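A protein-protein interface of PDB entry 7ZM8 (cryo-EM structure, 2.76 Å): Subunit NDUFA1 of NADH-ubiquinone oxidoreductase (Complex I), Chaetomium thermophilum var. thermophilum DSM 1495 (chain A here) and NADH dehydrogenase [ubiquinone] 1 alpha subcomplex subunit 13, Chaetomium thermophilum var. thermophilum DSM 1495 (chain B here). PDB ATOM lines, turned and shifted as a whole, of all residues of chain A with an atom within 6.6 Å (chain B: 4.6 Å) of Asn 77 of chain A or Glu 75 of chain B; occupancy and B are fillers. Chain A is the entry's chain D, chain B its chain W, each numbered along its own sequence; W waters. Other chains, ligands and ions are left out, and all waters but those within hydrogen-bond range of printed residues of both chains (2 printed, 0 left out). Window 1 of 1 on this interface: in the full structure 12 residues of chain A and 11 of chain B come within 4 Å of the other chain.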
ATOM      1  N   ARG A  55     -25.408  10.150  -1.678  1.00  0.00           N
ATOM      2  CA  ARG A  55     -24.167   9.834  -2.426  1.00  0.00           C
ATOM      3  C   ARG A  55     -24.348  10.194  -3.904  1.00  0.00           C
ATOM      4  O   ARG A  55     -23.401  10.760  -4.475  1.00  0.00           O
ATOM      5  CB  ARG A  55     -23.786   8.365  -2.238  1.00  0.00           C
ATOM      6  CG  ARG A  55     -23.151   8.034  -0.898  1.00  0.00           C
ATOM      7  CD  ARG A  55     -22.812   6.560  -0.914  1.00  0.00           C
ATOM      8  NE  ARG A  55     -21.775   6.279  -1.893  1.00  0.00           N
ATOM      9  CZ  ARG A  55     -21.462   5.067  -2.327  1.00  0.00           C
ATOM     10  NH1 ARG A  55     -22.129   4.018  -1.886  1.00  0.00           N
ATOM     11  NH2 ARG A  55     -20.495   4.904  -3.210  1.00  0.00           N
ATOM     12  N   GLY A  72     -16.428   9.685  -9.329  1.00  0.00           N
ATOM     13  CA  GLY A  72     -16.244   9.993  -7.931  1.00  0.00           C
ATOM     14  C   GLY A  72     -17.241   9.338  -7.002  1.00  0.00           C
ATOM     15  O   GLY A  72     -17.078   9.431  -5.782  1.00  0.00           O
ATOM     16  N   PHE A  73     -18.270   8.681  -7.542  1.00  0.00           N
ATOM     17  CA  PHE A  73     -19.241   7.996  -6.700  1.00  0.00           C
ATOM     18  C   PHE A  73     -18.613   6.824  -5.956  1.00  0.00           C
ATOM     19  O   PHE A  73     -19.061   6.475  -4.858  1.00  0.00           O
ATOM     20  CB  PHE A  73     -20.424   7.523  -7.545  1.00  0.00           C
ATOM     21  CG  PHE A  73     -21.425   6.716  -6.779  1.00  0.00           C
ATOM     22  CD1 PHE A  73     -22.309   7.329  -5.911  1.00  0.00           C
ATOM     23  CD2 PHE A  73     -21.472   5.344  -6.915  1.00  0.00           C
ATOM     24  CE1 PHE A  73     -23.218   6.590  -5.195  1.00  0.00           C
ATOM     25  CE2 PHE A  73     -22.383   4.601  -6.205  1.00  0.00           C
ATOM     26  CZ  PHE A  73     -23.256   5.223  -5.342  1.00  0.00           C
ATOM     27  N   GLU A  74     -17.579   6.208  -6.523  1.00  0.00           N
ATOM     28  CA  GLU A  74     -16.917   5.097  -5.857  1.00  0.00           C
ATOM     29  C   GLU A  74     -16.030   5.536  -4.699  1.00  0.00           C
ATOM     30  O   GLU A  74     -15.361   4.688  -4.103  1.00  0.00           O
ATOM     31  CB  GLU A  74     -16.094   4.300  -6.866  1.00  0.00           C
ATOM     32  CG  GLU A  74     -14.825   4.992  -7.327  1.00  0.00           C
ATOM     33  CD  GLU A  74     -15.054   5.868  -8.533  1.00  0.00           C
ATOM     34  OE1 GLU A  74     -16.223   6.200  -8.815  1.00  0.00           O
ATOM     35  OE2 GLU A  74     -14.064   6.219  -9.206  1.00  0.00           O
ATOM     36  N   PHE A  75     -16.014   6.826  -4.359  1.00  0.00           N
ATOM     37  CA  PHE A  75     -15.198   7.343  -3.270  1.00  0.00           C
ATOM     38  C   PHE A  75     -15.983   8.005  -2.149  1.00  0.00           C
ATOM     39  O   PHE A  75     -15.458   8.107  -1.038  1.00  0.00           O
ATOM     40  CB  PHE A  75     -14.182   8.367  -3.797  1.00  0.00           C
ATOM     41  CG  PHE A  75     -13.243   7.819  -4.827  1.00  0.00           C
ATOM     42  CD1 PHE A  75     -12.276   6.900  -4.480  1.00  0.00           C
ATOM     43  CD2 PHE A  75     -13.327   8.228  -6.140  1.00  0.00           C
ATOM     44  CE1 PHE A  75     -11.417   6.399  -5.423  1.00  0.00           C
ATOM     45  CE2 PHE A  75     -12.469   7.731  -7.082  1.00  0.00           C
ATOM     46  CZ  PHE A  75     -11.514   6.814  -6.724  1.00  0.00           C
ATOM     47  N   ASN A  76     -17.213   8.449  -2.433  1.00  0.00           N
ATOM     48  CA  ASN A  76     -18.027   9.221  -1.452  1.00  0.00           C
ATOM     49  C   ASN A  76     -18.828   8.318  -0.506  1.00  0.00           C
ATOM     50  O   ASN A  76     -19.711   8.849   0.180  1.00  0.00           O
ATOM     51  CB  ASN A  76     -18.943  10.225  -2.157  1.00  0.00           C
ATOM     52  CG  ASN A  76     -19.889   9.612  -3.168  1.00  0.00           C
ATOM     53  OD1 ASN A  76     -20.137   8.412  -3.156  1.00  0.00           O
ATOM     54  ND2 ASN A  76     -20.439  10.437  -4.040  1.00  0.00           N
ATOM     55  N   ASN A  77     -18.524   7.022  -0.457  1.00  0.00           N
ATOM     56  CA  ASN A  77     -19.235   6.124   0.439  1.00  0.00           C
ATOM     57  C   ASN A  77     -18.880   6.463   1.879  1.00  0.00           C
ATOM     58  O   ASN A  77     -17.703   6.381   2.251  1.00  0.00           O
ATOM     59  CB  ASN A  77     -18.871   4.682   0.116  1.00  0.00           C
ATOM     60  CG  ASN A  77     -19.823   3.689   0.735  1.00  0.00           C
ATOM     61  OD1 ASN A  77     -20.965   4.012   1.043  1.00  0.00           O
ATOM     62  ND2 ASN A  77     -19.353   2.463   0.921  1.00  0.00           N
ATOM     63  N   PRO A  78     -19.834   6.903   2.734  1.00  0.00           N
ATOM     64  CA  PRO A  78     -19.472   7.395   4.051  1.00  0.00           C
ATOM     65  C   PRO A  78     -19.183   6.284   5.052  1.00  0.00           C
ATOM     66  O   PRO A  78     -20.003   5.416   5.221  1.00  0.00           O
ATOM     67  CB  PRO A  78     -20.681   8.224   4.504  1.00  0.00           C
ATOM     68  CG  PRO A  78     -21.667   8.177   3.359  1.00  0.00           C
ATOM     69  CD  PRO A  78     -21.299   6.945   2.568  1.00  0.00           C
ATOM     70  N   TRP A  79     -18.020   6.330   5.698  1.00  0.00           N
ATOM     71  CA  TRP A  79     -17.820   5.404   6.839  1.00  0.00           C
ATOM     72  C   TRP A  79     -17.880   6.220   8.123  1.00  0.00           C
ATOM     73  O   TRP A  79     -16.940   6.981   8.374  1.00  0.00           O
ATOM     74  CB  TRP A  79     -16.507   4.626   6.693  1.00  0.00           C
ATOM     75  CG  TRP A  79     -16.529   3.509   5.695  1.00  0.00           C
ATOM     76  CD1 TRP A  79     -17.432   3.313   4.692  1.00  0.00           C
ATOM     77  CD2 TRP A  79     -15.585   2.425   5.598  1.00  0.00           C
ATOM     78  NE1 TRP A  79     -17.121   2.187   3.983  1.00  0.00           N
ATOM     79  CE2 TRP A  79     -15.994   1.620   4.516  1.00  0.00           C
ATOM     80  CE3 TRP A  79     -14.440   2.060   6.312  1.00  0.00           C
ATOM     81  CZ2 TRP A  79     -15.301   0.472   4.139  1.00  0.00           C
ATOM     82  CZ3 TRP A  79     -13.754   0.927   5.939  1.00  0.00           C
ATOM     83  CH2 TRP A  79     -14.183   0.144   4.868  1.00  0.00           C
ATOM     84  N   LEU B  71     -26.348  -4.319  -4.459  1.00  0.00           N
ATOM     85  CA  LEU B  71     -25.974  -3.362  -3.404  1.00  0.00           C
ATOM     86  C   LEU B  71     -24.770  -3.894  -2.635  1.00  0.00           C
ATOM     87  O   LEU B  71     -23.921  -3.080  -2.286  1.00  0.00           O
ATOM     88  CB  LEU B  71     -27.187  -3.015  -2.532  1.00  0.00           C
ATOM     89  CG  LEU B  71     -28.160  -2.006  -3.127  1.00  0.00           C
ATOM     90  CD1 LEU B  71     -29.477  -2.016  -2.372  1.00  0.00           C
ATOM     91  CD2 LEU B  71     -27.550  -0.620  -3.147  1.00  0.00           C
ATOM     92  N   GLN B  72     -24.716  -5.197  -2.384  1.00  0.00           N
ATOM     93  CA  GLN B  72     -23.596  -5.798  -1.676  1.00  0.00           C
ATOM     94  C   GLN B  72     -22.334  -5.811  -2.527  1.00  0.00           C
ATOM     95  O   GLN B  72     -21.226  -5.737  -1.988  1.00  0.00           O
ATOM     96  CB  GLN B  72     -23.962  -7.216  -1.243  1.00  0.00           C
ATOM     97  CG  GLN B  72     -23.018  -7.824  -0.233  1.00  0.00           C
ATOM     98  CD  GLN B  72     -22.892  -6.996   1.020  1.00  0.00           C
ATOM     99  OE1 GLN B  72     -23.881  -6.693   1.678  1.00  0.00           O
ATOM    100  NE2 GLN B  72     -21.667  -6.625   1.361  1.00  0.00           N
ATOM    101  N   ALA B  73     -22.479  -5.915  -3.847  1.00  0.00           N
ATOM    102  CA  ALA B  73     -21.317  -5.935  -4.726  1.00  0.00           C
ATOM    103  C   ALA B  73     -20.594  -4.597  -4.714  1.00  0.00           C
ATOM    104  O   ALA B  73     -19.360  -4.550  -4.700  1.00  0.00           O
ATOM    105  CB  ALA B  73     -21.746  -6.308  -6.141  1.00  0.00           C
ATOM    106  N   GLU B  74     -21.349  -3.497  -4.717  1.00  0.00           N
ATOM    107  CA  GLU B  74     -20.746  -2.173  -4.671  1.00  0.00           C
ATOM    108  C   GLU B  74     -20.116  -1.910  -3.311  1.00  0.00           C
ATOM    109  O   GLU B  74     -19.099  -1.215  -3.213  1.00  0.00           O
ATOM    110  CB  GLU B  74     -21.811  -1.128  -5.018  1.00  0.00           C
ATOM    111  CG  GLU B  74     -21.340   0.305  -5.251  1.00  0.00           C
ATOM    112  CD  GLU B  74     -21.186   1.103  -3.974  1.00  0.00           C
ATOM    113  OE1 GLU B  74     -21.908   0.812  -3.000  1.00  0.00           O
ATOM    114  OE2 GLU B  74     -20.344   2.026  -3.935  1.00  0.00           O
ATOM    115  N   GLU B  75     -20.698  -2.473  -2.254  1.00  0.00           N
ATOM    116  CA  GLU B  75     -20.082  -2.408  -0.935  1.00  0.00           C
ATOM    117  C   GLU B  75     -18.795  -3.225  -0.881  1.00  0.00           C
ATOM    118  O   GLU B  75     -17.820  -2.814  -0.244  1.00  0.00           O
ATOM    119  CB  GLU B  75     -21.074  -2.891   0.118  1.00  0.00           C
ATOM    120  CG  GLU B  75     -20.732  -2.509   1.558  1.00  0.00           C
ATOM    121  CD  GLU B  75     -20.912  -1.027   1.854  1.00  0.00           C
ATOM    122  OE1 GLU B  75     -21.693  -0.356   1.142  1.00  0.00           O
ATOM    123  OE2 GLU B  75     -20.276  -0.535   2.810  1.00  0.00           O
ATOM    124  N   ASP B  76     -18.773  -4.380  -1.552  1.00  0.00           N
ATOM    125  CA  ASP B  76     -17.620  -5.272  -1.481  1.00  0.00           C
ATOM    126  C   ASP B  76     -16.401  -4.681  -2.173  1.00  0.00           C
ATOM    127  O   ASP B  76     -15.269  -4.885  -1.723  1.00  0.00           O
ATOM    128  CB  ASP B  76     -17.964  -6.625  -2.088  1.00  0.00           C
ATOM    129  CG  ASP B  76     -18.831  -7.451  -1.186  1.00  0.00           C
ATOM    130  OD1 ASP B  76     -19.006  -7.051  -0.020  1.00  0.00           O
ATOM    131  OD2 ASP B  76     -19.336  -8.501  -1.634  1.00  0.00           O
ATOM    132  N   ARG B  77     -16.603  -3.973  -3.282  1.00  0.00           N
ATOM    133  CA  ARG B  77     -15.477  -3.312  -3.927  1.00  0.00           C
ATOM    134  C   ARG B  77     -14.936  -2.193  -3.054  1.00  0.00           C
ATOM    135  O   ARG B  77     -13.729  -1.936  -3.040  1.00  0.00           O
ATOM    136  CB  ARG B  77     -15.890  -2.781  -5.294  1.00  0.00           C
ATOM    137  CG  ARG B  77     -16.229  -3.861  -6.278  1.00  0.00           C
ATOM    138  CD  ARG B  77     -16.646  -3.295  -7.608  1.00  0.00           C
ATOM    139  NE  ARG B  77     -17.998  -2.753  -7.587  1.00  0.00           N
ATOM    140  CZ  ARG B  77     -19.064  -3.381  -8.069  1.00  0.00           C
ATOM    141  NH1 ARG B  77     -18.950  -4.585  -8.606  1.00  0.00           N
ATOM    142  NH2 ARG B  77     -20.250  -2.802  -8.010  1.00  0.00           N
ATOM    143  N   ASP B  78     -15.818  -1.520  -2.319  1.00  0.00           N
ATOM    144  CA  ASP B  78     -15.385  -0.462  -1.419  1.00  0.00           C
ATOM    145  C   ASP B  78     -14.577  -1.025  -0.258  1.00  0.00           C
ATOM    146  O   ASP B  78     -13.589  -0.421   0.167  1.00  0.00           O
ATOM    147  CB  ASP B  78     -16.601   0.304  -0.909  1.00  0.00           C
ATOM    148  CG  ASP B  78     -16.268   1.711  -0.488  1.00  0.00           C
ATOM    149  OD1 ASP B  78     -15.845   2.499  -1.355  1.00  0.00           O
ATOM    150  OD2 ASP B  78     -16.439   2.034   0.704  1.00  0.00           O
ATOM    151  N   HIS B  79     -14.965  -2.183   0.256  1.00  0.00           N
ATOM    152  CA  HIS B  79     -14.213  -2.840   1.348  1.00  0.00           C
ATOM    153  C   HIS B  79     -12.882  -3.348   0.812  1.00  0.00           C
ATOM    154  O   HIS B  79     -11.895  -3.257   1.540  1.00  0.00           O
ATOM    155  CB  HIS B  79     -15.048  -3.944   1.990  1.00  0.00           C
ATOM    156  CG  HIS B  79     -16.106  -3.421   2.890  1.00  0.00           C
ATOM    157  ND1 HIS B  79     -16.064  -3.597   4.248  1.00  0.00           N
ATOM    158  CD2 HIS B  79     -17.217  -2.702   2.634  1.00  0.00           C
ATOM    159  CE1 HIS B  79     -17.116  -3.033   4.785  1.00  0.00           C
ATOM    160  NE2 HIS B  79     -17.833  -2.471   3.824  1.00  0.00           N
ATOM    161  N   ARG B  82     -10.568   0.011   0.370  1.00  0.00           N
ATOM    162  CA  ARG B  82      -9.968   0.646   1.566  1.00  0.00           C
ATOM    163  C   ARG B  82      -8.954  -0.266   2.225  1.00  0.00           C
ATOM    164  O   ARG B  82      -8.015   0.251   2.818  1.00  0.00           O
ATOM    165  CB  ARG B  82     -11.117   1.096   2.474  1.00  0.00           C
ATOM    166  CG  ARG B  82     -12.069   2.048   1.764  1.00  0.00           C
ATOM    167  CD  ARG B  82     -13.017   2.845   2.630  1.00  0.00           C
ATOM    168  NE  ARG B  82     -12.346   3.583   3.683  1.00  0.00           N
ATOM    169  CZ  ARG B  82     -12.839   4.666   4.259  1.00  0.00           C
ATOM    170  NH1 ARG B  82     -12.162   5.275   5.213  1.00  0.00           N
ATOM    171  NH2 ARG B  82     -13.999   5.150   3.865  1.00  0.00           N
HETATM  172  O   HOH W   1     -24.078   2.398  -1.077  1.00  0.00           O
HETATM  173  O   HOH W   2     -20.228   1.286  -1.217  1.00  0.00           O
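The side-chain carboxylate (OD2) of Asp 78 of chain B lies within hydrogen-bond range of the indole nitrogen (NE1) of Trp 79 of chain A, at 3.4 Å.
The guanidinium group (NH2) of Arg 55 of chain A is in salt-bridge range of the side-chain carboxylate (OE2) of Glu 74 of chain B, at 3.0 Å.
The side-chain carboxylate (OD2) of Asp 78 of chain B sits at hydrogen-bond distance from the side-chain amide nitrogen (ND2) of Asn 77 of chain A (3.0 Å).
The backbone carbonyl oxygen of Phe 73 of chain A lies within hydrogen-bond range of the guanidinium group of Arg 55 of chain A.
The guanidinium group of Arg 55 of chain A sits at hydrogen-bond distance from the side-chain amide oxygen of Asn 77 of chain A (3.2 Å).
O of Phe 73 of chain A lies close to OD1 of Asn 76 of chain A, at 2.8 Å.
The side-chain carboxylate (OE2) of Glu 75 of chain B lies within hydrogen-bond range of a ring nitrogen (NE2) of His 79 of chain B (3.3 Å).
The guanidinium group (NE) of Arg 55 of chain A lies within hydrogen-bond range of the side-chain amide oxygen (OD1) of Asn 76 of chain A, at 3.0 Å.
Of chain B, only Glu 75 and Asp 78 come within 4 Å of Asn 77 of chain A.
Of chain A, only Asn 77 (3.7 Å) comes within 4 Å of Glu 75 of chain B.
Printed residues of chain B within 4 Å of Glu 74 of chain A: Asp 78 (3.5 Å).
Printed residues of chain B within 4 Å of Arg 55 of chain A: Glu 74 (3.0 Å).
Of the printed residues of chain A, Arg 82 of chain B touches Trp 79.
Printed residues of chain B within 4 Å of Phe 73 of chain A: Glu 74 (3.99 Å).
The nearest printed residue of chain A that does not touch Asp 78 of chain B is Phe 75 of chain A (5.2 Å).
Among the printed residues, merely in contact across the chains: Phe 73 of chain A with Glu 74 of chain B (3.99 Å), Glu 74 of chain A with Asp 78 of chain B (3.5 Å), Asn 77 of chain A with Glu 75 of chain B (3.7 Å), Trp 79 of chain A with His 79 of chain B (3.9 Å) and Trp 79 of chain A with Arg 82 of chain B (3.5 Å).
Water W2 lies within hydrogen-bond range of OE1 of Glu 74 of chain B (2.5 Å), ND2 of Asn 77 of chain A (2.6 Å), OE1 of Glu 75 of chain B (3.2 Å) and NH1 of Arg 55 of chain A (3.4 Å).
Water W1 lies within hydrogen-bond range of NH1 of Arg 55 of chain A (2.7 Å) and OE1 of Glu 74 of chain B (3.3 Å).
Of the 10 printed residues of chain B, 5 touch a printed residue of chain A.
Printed residues of chain B that touch a printed residue of chain A: Glu 74, Glu 75, Asp 78, His 79 and Arg 82.
Among the printed residues, 8 pairs touch across the chains.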
